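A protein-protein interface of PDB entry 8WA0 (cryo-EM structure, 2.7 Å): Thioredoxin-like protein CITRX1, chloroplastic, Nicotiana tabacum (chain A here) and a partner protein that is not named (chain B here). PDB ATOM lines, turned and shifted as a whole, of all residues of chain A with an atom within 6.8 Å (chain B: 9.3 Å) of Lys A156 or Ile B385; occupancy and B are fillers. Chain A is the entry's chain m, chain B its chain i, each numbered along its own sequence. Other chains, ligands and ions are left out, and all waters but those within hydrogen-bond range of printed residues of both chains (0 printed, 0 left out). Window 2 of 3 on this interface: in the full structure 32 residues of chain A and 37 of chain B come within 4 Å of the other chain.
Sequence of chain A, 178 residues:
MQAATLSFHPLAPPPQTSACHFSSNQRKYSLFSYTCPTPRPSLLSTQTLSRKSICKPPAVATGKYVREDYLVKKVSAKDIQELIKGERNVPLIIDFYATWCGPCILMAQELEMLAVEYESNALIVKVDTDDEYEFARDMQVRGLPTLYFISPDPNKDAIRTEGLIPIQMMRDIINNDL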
ATOM      1  N   ILE A  84     -23.383  -4.240  21.190  1.00  0.00           N
ATOM      2  CA  ILE A  84     -22.832  -5.534  20.868  1.00  0.00           C
ATOM      3  C   ILE A  84     -22.794  -5.725  19.356  1.00  0.00           C
ATOM      4  O   ILE A  84     -21.817  -6.247  18.823  1.00  0.00           O
ATOM      5  CB  ILE A  84     -23.511  -6.690  21.626  1.00  0.00           C
ATOM      6  CG1 ILE A  84     -22.550  -7.872  21.769  1.00  0.00           C
ATOM      7  CG2 ILE A  84     -24.818  -7.130  20.979  1.00  0.00           C
ATOM      8  CD1 ILE A  84     -21.308  -7.552  22.573  1.00  0.00           C
ATOM      9  N   MET A 139     -27.974 -12.611  30.452  1.00  0.00           N
ATOM     10  CA  MET A 139     -26.553 -12.580  30.326  1.00  0.00           C
ATOM     11  C   MET A 139     -25.975 -13.356  31.484  1.00  0.00           C
ATOM     12  O   MET A 139     -24.804 -13.234  31.792  1.00  0.00           O
ATOM     13  CB  MET A 139     -26.047 -11.165  30.212  1.00  0.00           C
ATOM     14  CG  MET A 139     -24.663 -11.012  29.628  1.00  0.00           C
ATOM     15  SD  MET A 139     -24.508  -9.411  28.832  1.00  0.00           S
ATOM     16  CE  MET A 139     -25.590  -9.655  27.428  1.00  0.00           C
ATOM     17  N   ILE A 150     -15.525  -7.889  27.603  1.00  0.00           N
ATOM     18  CA  ILE A 150     -15.747  -8.307  26.211  1.00  0.00           C
ATOM     19  C   ILE A 150     -14.756  -7.738  25.243  1.00  0.00           C
ATOM     20  O   ILE A 150     -14.103  -6.762  25.552  1.00  0.00           O
ATOM     21  CB  ILE A 150     -17.167  -8.074  25.717  1.00  0.00           C
ATOM     22  CG1 ILE A 150     -17.613  -6.652  26.032  1.00  0.00           C
ATOM     23  CG2 ILE A 150     -18.133  -9.048  26.358  1.00  0.00           C
ATOM     24  CD1 ILE A 150     -19.064  -6.392  25.702  1.00  0.00           C
ATOM     25  N   SER A 151     -14.615  -8.338  24.072  1.00  0.00           N
ATOM     26  CA  SER A 151     -13.566  -7.939  23.128  1.00  0.00           C
ATOM     27  C   SER A 151     -13.962  -7.555  21.715  1.00  0.00           C
ATOM     28  O   SER A 151     -15.022  -7.944  21.243  1.00  0.00           O
ATOM     29  CB  SER A 151     -12.564  -9.083  23.003  1.00  0.00           C
ATOM     30  OG  SER A 151     -11.952  -9.365  24.249  1.00  0.00           O
ATOM     31  N   PRO A 152     -13.073  -6.739  21.023  1.00  0.00           N
ATOM     32  CA  PRO A 152     -13.392  -6.408  19.629  1.00  0.00           C
ATOM     33  C   PRO A 152     -13.492  -7.559  18.644  1.00  0.00           C
ATOM     34  O   PRO A 152     -14.459  -7.591  17.894  1.00  0.00           O
ATOM     35  CB  PRO A 152     -12.200  -5.565  19.215  1.00  0.00           C
ATOM     36  CG  PRO A 152     -11.846  -4.832  20.439  1.00  0.00           C
ATOM     37  CD  PRO A 152     -11.865  -5.948  21.418  1.00  0.00           C
ATOM     38  N   ASP A 153     -12.503  -8.445  18.605  1.00  0.00           N
ATOM     39  CA  ASP A 153     -12.544  -9.610  17.727  1.00  0.00           C
ATOM     40  C   ASP A 153     -13.676 -10.491  18.119  1.00  0.00           C
ATOM     41  O   ASP A 153     -13.643 -11.094  19.180  1.00  0.00           O
ATOM     42  CB  ASP A 153     -11.252 -10.395  17.845  1.00  0.00           C
ATOM     43  N   PRO A 154     -14.679 -10.610  17.263  1.00  0.00           N
ATOM     44  CA  PRO A 154     -15.861 -11.348  17.680  1.00  0.00           C
ATOM     45  C   PRO A 154     -15.749 -12.825  17.505  1.00  0.00           C
ATOM     46  O   PRO A 154     -16.714 -13.456  17.101  1.00  0.00           O
ATOM     47  CB  PRO A 154     -16.955 -10.769  16.793  1.00  0.00           C
ATOM     48  CG  PRO A 154     -16.245 -10.211  15.593  1.00  0.00           C
ATOM     49  CD  PRO A 154     -14.762 -10.214  15.851  1.00  0.00           C
ATOM     50  N   ASN A 155     -14.601 -13.382  17.818  1.00  0.00           N
ATOM     51  CA  ASN A 155     -14.454 -14.803  17.777  1.00  0.00           C
ATOM     52  C   ASN A 155     -13.829 -15.120  19.108  1.00  0.00           C
ATOM     53  O   ASN A 155     -14.086 -16.175  19.678  1.00  0.00           O
ATOM     54  CB  ASN A 155     -13.522 -15.201  16.653  1.00  0.00           C
ATOM     55  N   LYS A 156     -13.008 -14.204  19.622  1.00  0.00           N
ATOM     56  CA  LYS A 156     -12.424 -14.395  20.949  1.00  0.00           C
ATOM     57  C   LYS A 156     -13.555 -14.264  21.939  1.00  0.00           C
ATOM     58  O   LYS A 156     -14.495 -13.508  21.715  1.00  0.00           O
ATOM     59  CB  LYS A 156     -11.316 -13.396  21.222  1.00  0.00           C
ATOM     60  CG  LYS A 156     -10.032 -14.018  21.727  1.00  0.00           C
ATOM     61  CD  LYS A 156      -8.946 -12.969  21.885  1.00  0.00           C
ATOM     62  CE  LYS A 156      -9.413 -11.616  21.375  1.00  0.00           C
ATOM     63  NZ  LYS A 156      -9.188 -10.537  22.377  1.00  0.00           N
ATOM     64  N   ASP A 157     -13.479 -14.973  23.049  1.00  0.00           N
ATOM     65  CA  ASP A 157     -14.605 -14.981  23.950  1.00  0.00           C
ATOM     66  C   ASP A 157     -14.696 -13.918  24.999  1.00  0.00           C
ATOM     67  O   ASP A 157     -13.885 -13.002  25.046  1.00  0.00           O
ATOM     68  CB  ASP A 157     -14.694 -16.341  24.611  1.00  0.00           C
ATOM     69  CG  ASP A 157     -15.652 -17.259  23.895  1.00  0.00           C
ATOM     70  OD1 ASP A 157     -16.467 -16.752  23.098  1.00  0.00           O
ATOM     71  OD2 ASP A 157     -15.591 -18.482  24.122  1.00  0.00           O
ATOM     72  N   ALA A 158     -15.704 -14.035  25.846  1.00  0.00           N
ATOM     73  CA  ALA A 158     -15.890 -13.081  26.944  1.00  0.00           C
ATOM     74  C   ALA A 158     -15.404 -13.599  28.272  1.00  0.00           C
ATOM     75  O   ALA A 158     -15.271 -14.804  28.439  1.00  0.00           O
ATOM     76  CB  ALA A 158     -17.350 -12.756  27.054  1.00  0.00           C
ATOM     77  N   ASN A 176      -4.324  -8.970  28.198  1.00  0.00           N
ATOM     78  CA  ASN A 176      -4.063 -10.295  27.630  1.00  0.00           C
ATOM     79  C   ASN A 176      -5.259 -11.119  27.288  1.00  0.00           C
ATOM     80  O   ASN A 176      -5.153 -12.321  27.302  1.00  0.00           O
ATOM     81  CB  ASN A 176      -3.149 -11.098  28.518  1.00  0.00           C
ATOM     82  CG  ASN A 176      -1.854 -10.382  28.831  1.00  0.00           C
ATOM     83  OD1 ASN A 176      -1.843  -9.352  29.498  1.00  0.00           O
ATOM     84  ND2 ASN A 176      -0.748 -10.943  28.369  1.00  0.00           N
ATOM     85  N   ASP A 177      -6.406 -10.501  27.074  1.00  0.00           N
ATOM     86  CA  ASP A 177      -7.619 -11.200  26.629  1.00  0.00           C
ATOM     87  C   ASP A 177      -8.682 -10.182  26.228  1.00  0.00           C
ATOM     88  O   ASP A 177      -9.813 -10.217  26.677  1.00  0.00           O
ATOM     89  CB  ASP A 177      -8.172 -12.156  27.653  1.00  0.00           C
ATOM     90  CG  ASP A 177      -8.979 -13.273  27.031  1.00  0.00           C
ATOM     91  OD1 ASP A 177      -9.204 -13.235  25.804  1.00  0.00           O
ATOM     92  OD2 ASP A 177      -9.384 -14.195  27.764  1.00  0.00           O
ATOM     93  N   HIS B 382     -14.749 -18.193  31.202  1.00  0.00           N
ATOM     94  CA  HIS B 382     -14.854 -17.831  29.796  1.00  0.00           C
ATOM     95  C   HIS B 382     -16.221 -18.201  29.279  1.00  0.00           C
ATOM     96  O   HIS B 382     -16.694 -19.303  29.517  1.00  0.00           O
ATOM     97  CB  HIS B 382     -13.767 -18.502  28.984  1.00  0.00           C
ATOM     98  CG  HIS B 382     -12.386 -18.109  29.395  1.00  0.00           C
ATOM     99  ND1 HIS B 382     -11.720 -17.040  28.836  1.00  0.00           N
ATOM    100  CD2 HIS B 382     -11.546 -18.635  30.316  1.00  0.00           C
ATOM    101  CE1 HIS B 382     -10.528 -16.928  29.392  1.00  0.00           C
ATOM    102  NE2 HIS B 382     -10.397 -17.883  30.295  1.00  0.00           N
ATOM    103  N   MET B 383     -16.862 -17.293  28.561  1.00  0.00           N
ATOM    104  CA  MET B 383     -18.218 -17.544  28.106  1.00  0.00           C
ATOM    105  C   MET B 383     -18.443 -17.237  26.645  1.00  0.00           C
ATOM    106  O   MET B 383     -17.880 -16.284  26.117  1.00  0.00           O
ATOM    107  CB  MET B 383     -19.200 -16.713  28.911  1.00  0.00           C
ATOM    108  CG  MET B 383     -19.295 -17.087  30.376  1.00  0.00           C
ATOM    109  SD  MET B 383     -20.824 -16.467  31.083  1.00  0.00           S
ATOM    110  CE  MET B 383     -20.690 -14.747  30.620  1.00  0.00           C
ATOM    111  N   LYS B 384     -19.269 -18.035  25.986  1.00  0.00           N
ATOM    112  CA  LYS B 384     -19.597 -17.785  24.590  1.00  0.00           C
ATOM    113  C   LYS B 384     -20.497 -16.584  24.476  1.00  0.00           C
ATOM    114  O   LYS B 384     -21.352 -16.380  25.324  1.00  0.00           O
ATOM    115  CB  LYS B 384     -20.298 -18.990  23.988  1.00  0.00           C
ATOM    116  N   ILE B 385     -20.343 -15.809  23.410  1.00  0.00           N
ATOM    117  CA  ILE B 385     -21.122 -14.585  23.259  1.00  0.00           C
ATOM    118  C   ILE B 385     -22.589 -14.935  23.188  1.00  0.00           C
ATOM    119  O   ILE B 385     -23.428 -14.256  23.777  1.00  0.00           O
ATOM    120  CB  ILE B 385     -20.654 -13.746  22.050  1.00  0.00           C
ATOM    121  CG1 ILE B 385     -19.538 -12.781  22.468  1.00  0.00           C
ATOM    122  CG2 ILE B 385     -21.792 -12.933  21.455  1.00  0.00           C
ATOM    123  CD1 ILE B 385     -18.193 -13.429  22.722  1.00  0.00           C
ATOM    124  N   GLY B 386     -22.914 -16.012  22.500  1.00  0.00           N
ATOM    125  CA  GLY B 386     -24.291 -16.453  22.490  1.00  0.00           C
ATOM    126  C   GLY B 386     -25.245 -15.918  21.455  1.00  0.00           C
ATOM    127  O   GLY B 386     -24.850 -15.164  20.568  1.00  0.00           O
ATOM    128  N   LYS B 387     -26.514 -16.304  21.565  1.00  0.00           N
ATOM    129  CA  LYS B 387     -27.518 -15.917  20.571  1.00  0.00           C
ATOM    130  C   LYS B 387     -28.007 -14.498  20.700  1.00  0.00           C
ATOM    131  O   LYS B 387     -27.689 -13.811  21.670  1.00  0.00           O
ATOM    132  CB  LYS B 387     -28.719 -16.866  20.621  1.00  0.00           C
ATOM    133  N   ARG B 388     -28.789 -14.057  19.718  1.00  0.00           N
ATOM    134  CA  ARG B 388     -29.333 -12.711  19.755  1.00  0.00           C
ATOM    135  C   ARG B 388     -30.150 -12.599  21.013  1.00  0.00           C
ATOM    136  O   ARG B 388     -30.831 -13.548  21.405  1.00  0.00           O
ATOM    137  CB  ARG B 388     -30.200 -12.443  18.529  1.00  0.00           C
ATOM    138  N   GLY B 389     -30.120 -11.437  21.650  1.00  0.00           N
ATOM    139  CA  GLY B 389     -30.771 -11.300  22.940  1.00  0.00           C
ATOM    140  C   GLY B 389     -29.676 -11.492  23.962  1.00  0.00           C
ATOM    141  O   GLY B 389     -29.937 -11.564  25.157  1.00  0.00           O
ATOM    142  N   GLY B 390     -28.442 -11.598  23.492  1.00  0.00           N
ATOM    143  CA  GLY B 390     -27.323 -11.722  24.396  1.00  0.00           C
ATOM    144  C   GLY B 390     -27.411 -12.892  25.352  1.00  0.00           C
ATOM    145  O   GLY B 390     -27.013 -12.766  26.505  1.00  0.00           O
ATOM    146  N   LEU B 391     -27.904 -14.038  24.905  1.00  0.00           N
ATOM    147  CA  LEU B 391     -28.036 -15.126  25.839  1.00  0.00           C
ATOM    148  C   LEU B 391     -26.697 -15.813  25.847  1.00  0.00           C
ATOM    149  O   LEU B 391     -26.384 -16.575  24.945  1.00  0.00           O
ATOM    150  CB  LEU B 391     -29.138 -16.075  25.399  1.00  0.00           C
ATOM    151  CG  LEU B 391     -29.401 -17.317  26.253  1.00  0.00           C
ATOM    152  CD1 LEU B 391     -29.821 -16.938  27.663  1.00  0.00           C
ATOM    153  CD2 LEU B 391     -30.457 -18.190  25.598  1.00  0.00           C
ATOM    154  N   ARG B 392     -25.897 -15.546  26.867  1.00  0.00           N
ATOM    155  CA  ARG B 392     -24.559 -16.106  26.927  1.00  0.00           C
ATOM    156  C   ARG B 392     -24.538 -17.574  27.256  1.00  0.00           C
ATOM    157  O   ARG B 392     -25.464 -18.085  27.877  1.00  0.00           O
ATOM    158  CB  ARG B 392     -23.733 -15.356  27.952  1.00  0.00           C
ATOM    159  CG  ARG B 392     -23.477 -13.900  27.622  1.00  0.00           C
ATOM    160  CD  ARG B 392     -22.068 -13.712  27.093  1.00  0.00           C
ATOM    161  NE  ARG B 392     -21.631 -12.324  27.178  1.00  0.00           N
ATOM    162  CZ  ARG B 392     -21.781 -11.430  26.207  1.00  0.00           C
ATOM    163  NH1 ARG B 392     -22.359 -11.772  25.064  1.00  0.00           N
ATOM    164  NH2 ARG B 392     -21.352 -10.189  26.380  1.00  0.00           N
ATOM    165  N   MET B 393     -23.493 -18.269  26.835  1.00  0.00           N
ATOM    166  CA  MET B 393     -23.346 -19.671  27.189  1.00  0.00           C
ATOM    167  C   MET B 393     -22.100 -19.708  28.017  1.00  0.00           C
ATOM    168  O   MET B 393     -21.090 -19.149  27.627  1.00  0.00           O
ATOM    169  CB  MET B 393     -23.178 -20.538  25.954  1.00  0.00           C
ATOM    170  N   THR B 394     -22.151 -20.352  29.165  1.00  0.00           N
ATOM    171  CA  THR B 394     -21.011 -20.304  30.067  1.00  0.00           C
ATOM    172  C   THR B 394     -20.115 -21.496  29.990  1.00  0.00           C
ATOM    173  O   THR B 394     -19.195 -21.644  30.791  1.00  0.00           O
ATOM    174  CB  THR B 394     -21.482 -20.165  31.522  1.00  0.00           C
ATOM    175  N   THR B 395     -20.361 -22.354  29.029  1.00  0.00           N
ATOM    176  CA  THR B 395     -19.601 -23.581  28.997  1.00  0.00           C
ATOM    177  C   THR B 395     -18.284 -23.488  28.274  1.00  0.00           C
ATOM    178  O   THR B 395     -17.570 -24.482  28.197  1.00  0.00           O
ATOM    179  CB  THR B 395     -20.421 -24.742  28.409  1.00  0.00           C
ATOM    180  N   THR B 396     -17.930 -22.322  27.750  1.00  0.00           N
ATOM    181  CA  THR B 396     -16.710 -22.284  26.971  1.00  0.00           C
ATOM    182  C   THR B 396     -15.597 -22.733  27.886  1.00  0.00           C
ATOM    183  O   THR B 396     -14.773 -23.544  27.482  1.00  0.00           O
ATOM    184  CB  THR B 396     -16.439 -20.890  26.406  1.00  0.00           C
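N of Lys B384 lies within hydrogen-bond range of O of Met B393 (2.7 Å).
O of Ile B385 sits at hydrogen-bond distance from NH1 of Arg B392 (3.0 Å).
The side-chain hydroxyl (OG) of Ser A151 is in hydrogen-bond range of the backbone carbonyl oxygen (O) of Asp A177.
The backbone carbonyl oxygen (O) of Ala A158 is in hydrogen-bond range of the backbone NH (N) of Met B383 (3.0 Å).
OD1 of Asp A157 lies close to O of Met B383 (3.4 Å).
Of the 15 printed residues of chain B, 7 touch a printed residue of chain A.
Printed residues of chain B that touch a printed residue of chain A: His B382, Met B383, Lys B384, Ile B385, Gly B390, Arg B392 and Thr B396.
Printed residues of chain A that touch a printed residue of chain B: Met A139, Ile A150, Lys A156, Asp A157, Ala A158 and Asp A177.
Among the printed residues, no Asp or Glu carboxylate lies within 4 Å of a Lys or Arg side-chain nitrogen of the other chain.
Among the printed residues, merely in contact across the chains: Met A139 with Gly B390, Met A139 with Arg B392, Ile A150 with Arg B392, Lys A156 with Ile B385, Asp A157 with Lys B384, Asp A157 with Ile B385, Asp A157 with Thr B396, Ala A158 with His B382 and Asp A177 with His B382.
Printed residues of chain B within 4 Å of Met A139: Gly B390 (3.5 Å) and Arg B392 (3.7 Å).
Pro A154 touches none of the printed residues of chain B.
No residue of chain B comes within 4 Å of Asn A155.
Asp A157 touches just these residues of chain B: Met B383 (3.3 Å), Lys B384 (3.6 Å), Ile B385 (3.8 Å) and Thr B396 (3.4 Å).
Asn A176 touches none of the printed residues of chain B.
Ile B385 touches two residues of chain A.
Printed residues of chain A within 4 Å of Gly B390: Met A139 (3.5 Å).
Of the printed residues of chain A, Arg B392 touches Met A139 and Ile A150.
The nearest residue of chain A that does not touch Ile B385 is Ala A158 (4.04 Å).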
